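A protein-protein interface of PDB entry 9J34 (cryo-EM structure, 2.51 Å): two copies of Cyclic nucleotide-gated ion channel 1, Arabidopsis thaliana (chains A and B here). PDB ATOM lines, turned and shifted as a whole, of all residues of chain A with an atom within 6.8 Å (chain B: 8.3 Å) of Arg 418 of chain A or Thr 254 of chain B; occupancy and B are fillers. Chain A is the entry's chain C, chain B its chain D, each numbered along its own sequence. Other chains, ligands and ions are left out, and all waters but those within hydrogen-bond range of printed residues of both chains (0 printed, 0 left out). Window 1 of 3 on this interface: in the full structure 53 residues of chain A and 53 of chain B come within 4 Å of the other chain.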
ATOM      1  N   THR A 411      16.821  23.783  25.484  1.00  0.00           N
ATOM      2  CA  THR A 411      17.590  23.489  24.366  1.00  0.00           C
ATOM      3  C   THR A 411      18.684  22.465  24.533  1.00  0.00           C
ATOM      4  O   THR A 411      19.557  22.486  23.763  1.00  0.00           O
ATOM      5  CB  THR A 411      18.125  24.817  23.898  1.00  0.00           C
ATOM      6  OG1 THR A 411      18.892  25.431  24.929  1.00  0.00           O
ATOM      7  CG2 THR A 411      16.992  25.733  23.559  1.00  0.00           C
ATOM      8  N   ARG A 413      18.763  18.786  24.285  1.00  0.00           N
ATOM      9  CA  ARG A 413      18.847  17.636  23.372  1.00  0.00           C
ATOM     10  C   ARG A 413      19.225  18.210  22.039  1.00  0.00           C
ATOM     11  O   ARG A 413      19.824  17.529  21.301  1.00  0.00           O
ATOM     12  CB  ARG A 413      17.560  16.798  23.493  1.00  0.00           C
ATOM     13  CG  ARG A 413      17.478  15.941  24.740  1.00  0.00           C
ATOM     14  CD  ARG A 413      18.140  14.615  24.509  1.00  0.00           C
ATOM     15  NE  ARG A 413      18.134  13.820  25.716  1.00  0.00           N
ATOM     16  CZ  ARG A 413      18.793  14.127  26.823  1.00  0.00           C
ATOM     17  NH1 ARG A 413      19.531  15.221  26.887  1.00  0.00           N
ATOM     18  NH2 ARG A 413      18.711  13.335  27.873  1.00  0.00           N
ATOM     19  N   LEU A 414      19.068  19.489  21.922  1.00  0.00           N
ATOM     20  CA  LEU A 414      19.250  20.187  20.659  1.00  0.00           C
ATOM     21  C   LEU A 414      20.646  20.760  20.554  1.00  0.00           C
ATOM     22  O   LEU A 414      21.245  20.744  19.477  1.00  0.00           O
ATOM     23  CB  LEU A 414      18.203  21.297  20.513  1.00  0.00           C
ATOM     24  CG  LEU A 414      18.338  22.318  19.386  1.00  0.00           C
ATOM     25  CD1 LEU A 414      18.074  21.656  18.056  1.00  0.00           C
ATOM     26  CD2 LEU A 414      17.369  23.456  19.607  1.00  0.00           C
ATOM     27  N   GLU A 415      21.164  21.259  21.677  1.00  0.00           N
ATOM     28  CA  GLU A 415      22.602  21.423  21.838  1.00  0.00           C
ATOM     29  C   GLU A 415      23.366  20.128  21.630  1.00  0.00           C
ATOM     30  O   GLU A 415      24.399  20.121  20.950  1.00  0.00           O
ATOM     31  CB  GLU A 415      22.915  22.017  23.210  1.00  0.00           C
ATOM     32  CG  GLU A 415      24.358  22.339  23.272  1.00  0.00           C
ATOM     33  CD  GLU A 415      24.688  23.629  22.654  1.00  0.00           C
ATOM     34  OE1 GLU A 415      23.889  24.589  22.713  1.00  0.00           O
ATOM     35  OE2 GLU A 415      25.717  23.586  21.962  1.00  0.00           O
ATOM     36  N   GLU A 416      22.872  19.022  22.180  1.00  0.00           N
ATOM     37  CA  GLU A 416      23.602  17.763  22.088  1.00  0.00           C
ATOM     38  C   GLU A 416      23.626  17.244  20.654  1.00  0.00           C
ATOM     39  O   GLU A 416      24.589  16.590  20.243  1.00  0.00           O
ATOM     40  CB  GLU A 416      22.982  16.754  23.053  1.00  0.00           C
ATOM     41  CG  GLU A 416      23.653  15.405  23.114  1.00  0.00           C
ATOM     42  CD  GLU A 416      22.771  14.364  23.757  1.00  0.00           C
ATOM     43  OE1 GLU A 416      21.814  14.754  24.458  1.00  0.00           O
ATOM     44  OE2 GLU A 416      23.033  13.160  23.566  1.00  0.00           O
ATOM     45  N   MET A 417      22.601  17.572  19.866  1.00  0.00           N
ATOM     46  CA  MET A 417      22.610  17.223  18.450  1.00  0.00           C
ATOM     47  C   MET A 417      23.590  18.087  17.664  1.00  0.00           C
ATOM     48  O   MET A 417      24.246  17.598  16.737  1.00  0.00           O
ATOM     49  CB  MET A 417      21.200  17.352  17.875  1.00  0.00           C
ATOM     50  CG  MET A 417      21.046  16.833  16.454  1.00  0.00           C
ATOM     51  SD  MET A 417      21.167  18.104  15.179  1.00  0.00           S
ATOM     52  CE  MET A 417      20.034  19.331  15.810  1.00  0.00           C
ATOM     53  N   ARG A 418      23.693  19.375  18.008  1.00  0.00           N
ATOM     54  CA  ARG A 418      24.592  20.272  17.285  1.00  0.00           C
ATOM     55  C   ARG A 418      26.054  19.955  17.556  1.00  0.00           C
ATOM     56  O   ARG A 418      26.901  20.144  16.677  1.00  0.00           O
ATOM     57  CB  ARG A 418      24.312  21.725  17.654  1.00  0.00           C
ATOM     58  CG  ARG A 418      22.999  22.282  17.158  1.00  0.00           C
ATOM     59  CD  ARG A 418      22.963  23.781  17.385  1.00  0.00           C
ATOM     60  NE  ARG A 418      21.619  24.332  17.301  1.00  0.00           N
ATOM     61  CZ  ARG A 418      21.013  24.960  18.302  1.00  0.00           C
ATOM     62  NH1 ARG A 418      21.632  25.112  19.463  1.00  0.00           N
ATOM     63  NH2 ARG A 418      19.789  25.437  18.143  1.00  0.00           N
ATOM     64  N   VAL A 419      26.369  19.493  18.767  1.00  0.00           N
ATOM     65  CA  VAL A 419      27.732  19.089  19.085  1.00  0.00           C
ATOM     66  C   VAL A 419      28.087  17.805  18.346  1.00  0.00           C
ATOM     67  O   VAL A 419      29.198  17.661  17.825  1.00  0.00           O
ATOM     68  CB  VAL A 419      27.884  18.945  20.610  1.00  0.00           C
ATOM     69  CG1 VAL A 419      29.248  18.390  20.992  1.00  0.00           C
ATOM     70  CG2 VAL A 419      27.652  20.275  21.267  1.00  0.00           C
ATOM     71  N   LYS A 420      27.015  16.914  18.007  1.00  0.00           N
ATOM     72  CA  LYS A 420      27.218  15.660  17.291  1.00  0.00           C
ATOM     73  C   LYS A 420      27.302  15.872  15.787  1.00  0.00           C
ATOM     74  O   LYS A 420      28.014  15.137  15.098  1.00  0.00           O
ATOM     75  CB  LYS A 420      26.090  14.684  17.608  1.00  0.00           C
ATOM     76  CG  LYS A 420      26.171  14.045  18.971  1.00  0.00           C
ATOM     77  CD  LYS A 420      24.966  13.157  19.210  1.00  0.00           C
ATOM     78  CE  LYS A 420      24.849  12.769  20.672  1.00  0.00           C
ATOM     79  NZ  LYS A 420      23.655  11.915  20.914  1.00  0.00           N
ATOM     80  N   ARG A 421      26.574  16.859  15.263  1.00  0.00           N
ATOM     81  CA  ARG A 421      26.664  17.176  13.844  1.00  0.00           C
ATOM     82  C   ARG A 421      27.996  17.827  13.508  1.00  0.00           C
ATOM     83  O   ARG A 421      28.596  17.509  12.478  1.00  0.00           O
ATOM     84  CB  ARG A 421      25.510  18.086  13.441  1.00  0.00           C
ATOM     85  CG  ARG A 421      24.981  17.835  12.050  1.00  0.00           C
ATOM     86  CD  ARG A 421      23.685  18.580  11.844  1.00  0.00           C
ATOM     87  NE  ARG A 421      23.744  19.910  12.434  1.00  0.00           N
ATOM     88  CZ  ARG A 421      22.741  20.779  12.417  1.00  0.00           C
ATOM     89  NH1 ARG A 421      21.594  20.458  11.840  1.00  0.00           N
ATOM     90  NH2 ARG A 421      22.887  21.969  12.983  1.00  0.00           N
ATOM     91  N   ARG A 422      28.474  18.729  14.365  1.00  0.00           N
ATOM     92  CA  ARG A 422      29.804  19.304  14.226  1.00  0.00           C
ATOM     93  C   ARG A 422      30.912  18.314  14.543  1.00  0.00           C
ATOM     94  O   ARG A 422      32.066  18.585  14.207  1.00  0.00           O
ATOM     95  CB  ARG A 422      29.949  20.524  15.135  1.00  0.00           C
ATOM     96  CG  ARG A 422      29.280  21.774  14.613  1.00  0.00           C
ATOM     97  CD  ARG A 422      29.562  22.958  15.513  1.00  0.00           C
ATOM     98  NE  ARG A 422      28.414  23.285  16.353  1.00  0.00           N
ATOM     99  CZ  ARG A 422      28.428  23.242  17.678  1.00  0.00           C
ATOM    100  NH1 ARG A 422      29.530  22.895  18.323  1.00  0.00           N
ATOM    101  NH2 ARG A 422      27.337  23.555  18.364  1.00  0.00           N
ATOM    102  N   ASP A 423      30.603  17.207  15.214  1.00  0.00           N
ATOM    103  CA  ASP A 423      31.554  16.124  15.409  1.00  0.00           C
ATOM    104  C   ASP A 423      31.601  15.177  14.223  1.00  0.00           C
ATOM    105  O   ASP A 423      32.660  14.611  13.939  1.00  0.00           O
ATOM    106  CB  ASP A 423      31.210  15.326  16.670  1.00  0.00           C
ATOM    107  CG  ASP A 423      31.697  15.997  17.936  1.00  0.00           C
ATOM    108  OD1 ASP A 423      32.038  17.196  17.884  1.00  0.00           O
ATOM    109  OD2 ASP A 423      31.736  15.324  18.986  1.00  0.00           O
ATOM    110  N   THR B 252      12.594  27.607  11.328  1.00  0.00           N
ATOM    111  CA  THR B 252      13.817  26.823  11.186  1.00  0.00           C
ATOM    112  C   THR B 252      14.662  26.916  12.443  1.00  0.00           C
ATOM    113  O   THR B 252      14.313  27.623  13.385  1.00  0.00           O
ATOM    114  CB  THR B 252      14.662  27.297   9.993  1.00  0.00           C
ATOM    115  OG1 THR B 252      15.813  26.453   9.858  1.00  0.00           O
ATOM    116  CG2 THR B 252      15.116  28.734  10.204  1.00  0.00           C
ATOM    117  N   GLU B 253      15.777  26.192  12.460  1.00  0.00           N
ATOM    118  CA  GLU B 253      16.744  26.292  13.543  1.00  0.00           C
ATOM    119  C   GLU B 253      18.148  26.423  12.971  1.00  0.00           C
ATOM    120  O   GLU B 253      18.498  25.747  11.999  1.00  0.00           O
ATOM    121  CB  GLU B 253      16.641  25.099  14.506  1.00  0.00           C
ATOM    122  CG  GLU B 253      16.937  23.719  13.925  1.00  0.00           C
ATOM    123  CD  GLU B 253      18.388  23.311  14.084  1.00  0.00           C
ATOM    124  OE1 GLU B 253      19.138  24.029  14.780  1.00  0.00           O
ATOM    125  OE2 GLU B 253      18.780  22.277  13.504  1.00  0.00           O
ATOM    126  N   THR B 254      18.917  27.337  13.549  1.00  0.00           N
ATOM    127  CA  THR B 254      20.368  27.335  13.515  1.00  0.00           C
ATOM    128  C   THR B 254      20.831  27.709  14.912  1.00  0.00           C
ATOM    129  O   THR B 254      20.016  27.890  15.820  1.00  0.00           O
ATOM    130  CB  THR B 254      20.952  28.307  12.474  1.00  0.00           C
ATOM    131  OG1 THR B 254      20.172  29.504  12.430  1.00  0.00           O
ATOM    132  CG2 THR B 254      20.986  27.679  11.097  1.00  0.00           C
ATOM    133  N   ALA B 255      22.147  27.798  15.091  1.00  0.00           N
ATOM    134  CA  ALA B 255      22.673  28.213  16.385  1.00  0.00           C
ATOM    135  C   ALA B 255      22.363  29.674  16.688  1.00  0.00           C
ATOM    136  O   ALA B 255      22.221  30.035  17.861  1.00  0.00           O
ATOM    137  CB  ALA B 255      24.179  27.966  16.440  1.00  0.00           C
ATOM    138  N   TRP B 256      22.236  30.511  15.661  1.00  0.00           N
ATOM    139  CA  TRP B 256      22.021  31.940  15.831  1.00  0.00           C
ATOM    140  C   TRP B 256      20.594  32.383  15.538  1.00  0.00           C
ATOM    141  O   TRP B 256      20.321  33.586  15.592  1.00  0.00           O
ATOM    142  CB  TRP B 256      22.981  32.723  14.931  1.00  0.00           C
ATOM    143  CG  TRP B 256      22.989  32.242  13.516  1.00  0.00           C
ATOM    144  CD1 TRP B 256      23.850  31.342  12.970  1.00  0.00           C
ATOM    145  CD2 TRP B 256      22.100  32.637  12.463  1.00  0.00           C
ATOM    146  NE1 TRP B 256      23.553  31.146  11.645  1.00  0.00           N
ATOM    147  CE2 TRP B 256      22.484  31.931  11.309  1.00  0.00           C
ATOM    148  CE3 TRP B 256      21.018  33.521  12.384  1.00  0.00           C
ATOM    149  CZ2 TRP B 256      21.825  32.077  10.092  1.00  0.00           C
ATOM    150  CZ3 TRP B 256      20.364  33.662  11.178  1.00  0.00           C
ATOM    151  CH2 TRP B 256      20.770  32.944  10.047  1.00  0.00           C
ATOM    152  N   ALA B 257      19.688  31.459  15.208  1.00  0.00           N
ATOM    153  CA  ALA B 257      18.342  31.852  14.806  1.00  0.00           C
ATOM    154  C   ALA B 257      17.512  32.370  15.968  1.00  0.00           C
ATOM    155  O   ALA B 257      16.622  33.196  15.752  1.00  0.00           O
ATOM    156  CB  ALA B 257      17.617  30.683  14.146  1.00  0.00           C
ATOM    157  N   GLY B 258      17.778  31.907  17.190  1.00  0.00           N
ATOM    158  CA  GLY B 258      17.097  32.458  18.344  1.00  0.00           C
ATOM    159  C   GLY B 258      17.491  33.878  18.660  1.00  0.00           C
ATOM    160  O   GLY B 258      16.682  34.626  19.213  1.00  0.00           O
ATOM    161  N   ALA B 259      18.718  34.262  18.314  1.00  0.00           N
ATOM    162  CA  ALA B 259      19.195  35.628  18.456  1.00  0.00           C
ATOM    163  C   ALA B 259      18.774  36.525  17.301  1.00  0.00           C
ATOM    164  O   ALA B 259      18.522  37.715  17.516  1.00  0.00           O
ATOM    165  CB  ALA B 259      20.719  35.633  18.578  1.00  0.00           C
ATOM    166  N   ALA B 260      18.695  35.987  16.081  1.00  0.00           N
ATOM    167  CA  ALA B 260      18.247  36.786  14.946  1.00  0.00           C
ATOM    168  C   ALA B 260      16.748  37.045  14.996  1.00  0.00           C
ATOM    169  O   ALA B 260      16.290  38.105  14.560  1.00  0.00           O
ATOM    170  CB  ALA B 260      18.621  36.098  13.636  1.00  0.00           C
ATOM    171  N   ASN B 402      19.895  34.583  24.413  1.00  0.00           N
ATOM    172  CA  ASN B 402      19.952  34.036  23.110  1.00  0.00           C
ATOM    173  C   ASN B 402      21.258  34.159  22.482  1.00  0.00           C
ATOM    174  O   ASN B 402      21.541  33.527  21.556  1.00  0.00           O
ATOM    175  CB  ASN B 402      18.877  34.707  22.325  1.00  0.00           C
ATOM    176  CG  ASN B 402      17.617  33.950  22.342  1.00  0.00           C
ATOM    177  OD1 ASN B 402      17.614  32.771  22.113  1.00  0.00           O
ATOM    178  ND2 ASN B 402      16.542  34.602  22.619  1.00  0.00           N
ATOM    179  N   THR B 405      23.577  31.607  24.235  1.00  0.00           N
ATOM    180  CA  THR B 405      23.333  30.311  23.860  1.00  0.00           C
ATOM    181  C   THR B 405      24.082  30.164  22.594  1.00  0.00           C
ATOM    182  O   THR B 405      24.786  29.259  22.488  1.00  0.00           O
ATOM    183  CB  THR B 405      21.823  29.876  23.821  1.00  0.00           C
ATOM    184  OG1 THR B 405      21.131  30.514  22.752  1.00  0.00           O
ATOM    185  CG2 THR B 405      21.164  30.161  25.135  1.00  0.00           C
ATOM    186  N   TYR B 406      23.943  30.984  21.612  1.00  0.00           N
ATOM    187  CA  TYR B 406      24.745  30.858  20.475  1.00  0.00           C
ATOM    188  C   TYR B 406      26.205  30.667  20.796  1.00  0.00           C
ATOM    189  O   TYR B 406      26.840  29.879  20.177  1.00  0.00           O
ATOM    190  CB  TYR B 406      24.601  32.013  19.613  1.00  0.00           C
ATOM    191  CG  TYR B 406      25.532  32.089  18.492  1.00  0.00           C
ATOM    192  CD1 TYR B 406      25.463  31.196  17.460  1.00  0.00           C
ATOM    193  CD2 TYR B 406      26.480  33.075  18.449  1.00  0.00           C
ATOM    194  CE1 TYR B 406      26.321  31.277  16.406  1.00  0.00           C
ATOM    195  CE2 TYR B 406      27.350  33.164  17.404  1.00  0.00           C
ATOM    196  CZ  TYR B 406      27.257  32.261  16.388  1.00  0.00           C
ATOM    197  OH  TYR B 406      28.127  32.359  15.351  1.00  0.00           O
ATOM    198  N   GLN B 408      27.823  29.527  23.402  1.00  0.00           N
ATOM    199  CA  GLN B 408      28.155  28.329  24.031  1.00  0.00           C
ATOM    200  C   GLN B 408      27.860  27.135  23.182  1.00  0.00           C
ATOM    201  O   GLN B 408      28.332  26.089  23.441  1.00  0.00           O
ATOM    202  CB  GLN B 408      27.319  28.263  25.235  1.00  0.00           C
ATOM    203  CG  GLN B 408      27.930  28.717  26.510  1.00  0.00           C
ATOM    204  CD  GLN B 408      26.882  28.691  27.580  1.00  0.00           C
ATOM    205  OE1 GLN B 408      25.786  28.176  27.361  1.00  0.00           O
ATOM    206  NE2 GLN B 408      27.192  29.258  28.738  1.00  0.00           N
ATOM    207  N   SER B 409      27.073  27.248  22.192  1.00  0.00           N
ATOM    208  CA  SER B 409      26.814  26.176  21.338  1.00  0.00           C
ATOM    209  C   SER B 409      28.035  25.879  20.638  1.00  0.00           C
ATOM    210  O   SER B 409      28.353  24.747  20.359  1.00  0.00           O
ATOM    211  CB  SER B 409      25.774  26.592  20.331  1.00  0.00           C
ATOM    212  OG  SER B 409      26.237  27.625  19.499  1.00  0.00           O
ATOM    213  N   THR B 410      28.799  26.889  20.418  1.00  0.00           N
ATOM    214  CA  THR B 410      29.942  26.716  19.628  1.00  0.00           C
ATOM    215  C   THR B 410      31.186  26.283  20.363  1.00  0.00           C
ATOM    216  O   THR B 410      32.195  26.104  19.738  1.00  0.00           O
ATOM    217  CB  THR B 410      30.176  27.987  18.791  1.00  0.00           C
ATOM    218  OG1 THR B 410      30.341  29.126  19.639  1.00  0.00           O
ATOM    219  CG2 THR B 410      29.005  28.242  17.855  1.00  0.00           C
ATOM    220  N   THR B 412      31.434  23.501  23.065  1.00  0.00           N
ATOM    221  CA  THR B 412      31.263  22.325  23.948  1.00  0.00           C
ATOM    222  C   THR B 412      32.461  21.393  23.967  1.00  0.00           C
ATOM    223  O   THR B 412      32.846  21.029  25.039  1.00  0.00           O
ATOM    224  CB  THR B 412      29.972  21.560  23.589  1.00  0.00           C
ATOM    225  OG1 THR B 412      28.864  22.423  23.823  1.00  0.00           O
ATOM    226  CG2 THR B 412      29.789  20.254  24.323  1.00  0.00           C
ATOM    227  N   ARG B 413      33.241  21.109  22.853  1.00  0.00           N
ATOM    228  CA  ARG B 413      34.336  20.131  22.769  1.00  0.00           C
ATOM    229  C   ARG B 413      35.574  20.857  23.210  1.00  0.00           C
ATOM    230  O   ARG B 413      36.370  20.255  23.820  1.00  0.00           O
ATOM    231  CB  ARG B 413      34.310  19.482  21.372  1.00  0.00           C
ATOM    232  CG  ARG B 413      33.222  18.449  21.171  1.00  0.00           C
ATOM    233  CD  ARG B 413      33.705  17.108  21.636  1.00  0.00           C
ATOM    234  NE  ARG B 413      32.658  16.119  21.524  1.00  0.00           N
ATOM    235  CZ  ARG B 413      31.538  16.125  22.228  1.00  0.00           C
ATOM    236  NH1 ARG B 413      31.306  17.070  23.122  1.00  0.00           N
ATOM    237  NH2 ARG B 413      30.641  15.179  22.035  1.00  0.00           N
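Glu 415 of chain A touches Gln 408 of chain B (OE2 to O, 3.9 Å). OE2 of Glu 415 of chain A touches OG1 of Thr 412 of chain B (3.8 Å). Glu 253 of chain B touches Met 417 of chain A. CG2 of Val 419 of chain A touches CB of Thr 412 of chain B, at 3.5 Å. Val 419 of chain A touches Arg 413 of chain B.
Arg 418 of chain A touches just these residues of chain B: Glu 253 (3.6 Å) and Thr 254 (3.4 Å). Of the printed residues of chain B, Arg 422 of chain A touches Ser 409 (2.5 Å). Of the printed residues of chain A, Glu 253 of chain B touches Met 417 (3.9 Å), Arg 418 (3.6 Å) and Arg 421 (3.7 Å). Of the printed residues of chain A, Thr 254 of chain B touches Arg 418. Of the printed residues of chain A, Thr 412 of chain B touches Glu 415 and Val 419. The nearest residue of chain B that does not touch Arg 418 of chain A is Ala 255 of chain B (4.1 Å). The nearest printed residue of chain B that does not touch Glu 415 of chain A is Thr 405 of chain B (4.8 Å).
The side-chain carboxylate (OE2) of Glu 415 of chain A lies close to the backbone carbonyl oxygen (O) of Ser 409 of chain B (3.3 Å). The guanidinium group (NE) of Arg 413 of chain B lies within salt-bridge range of the side-chain carboxylate (OD2) of Asp 423 of chain A, 2.8 Å away. The guanidinium group (NE) of Arg 418 of chain A lies within salt-bridge range of the side-chain carboxylate (OE1) of Glu 253 of chain B (3.6 Å). The guanidinium group (NH2) of Arg 422 of chain A sits at hydrogen-bond distance from the backbone carbonyl oxygen (O) of Ser 409 of chain B (2.5 Å). OE2 of Glu 253 of chain B lies within salt-bridge range of NH1 of Arg 421 of chain A (3.7 Å). The guanidinium group (NH2) of Arg 418 of chain A is in hydrogen-bond range of the backbone carbonyl oxygen (O) of Thr 254 of chain B.
Position printed for both chains: 413. Of the 11 pairs that touch across the chains among the printed residues, none has its exchanged pair printed and touching as well.
Printed residues of chain B that touch a printed residue of chain A: Glu 253, Thr 254, Gln 408, Ser 409, Thr 412 and Arg 413. Of the 12 printed residues of chain A, 7 touch a printed residue of chain B. Among the printed residues, 11 pairs touch across the chains. Among the printed residues, Asp or Glu carboxylates within 4 Å of a Lys or Arg side-chain nitrogen of the other chain: Arg 418 of chain A with Glu 253 of chain B, Arg 421 of chain A with Glu 253 of chain B and Asp 423 of chain A with Arg 413 of chain B.
The side-chain carboxylate (OE1) of Glu 415 of chain A lies within salt-bridge range of the guanidinium group (NH1) of Arg 418 of chain A, 3.99 Å away. OG1 of Thr 254 of chain B sits close to N of Ala 257 of chain B (3.4 Å). OE2 of Glu 415 of chain A lies within salt-bridge range of NH2 of Arg 422 of chain A, 3.9 Å away. The backbone carbonyl oxygen (O) of Tyr 406 of chain B is in hydrogen-bond range of the side-chain hydroxyl (OG) of Ser 409 of chain B (2.4 Å).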
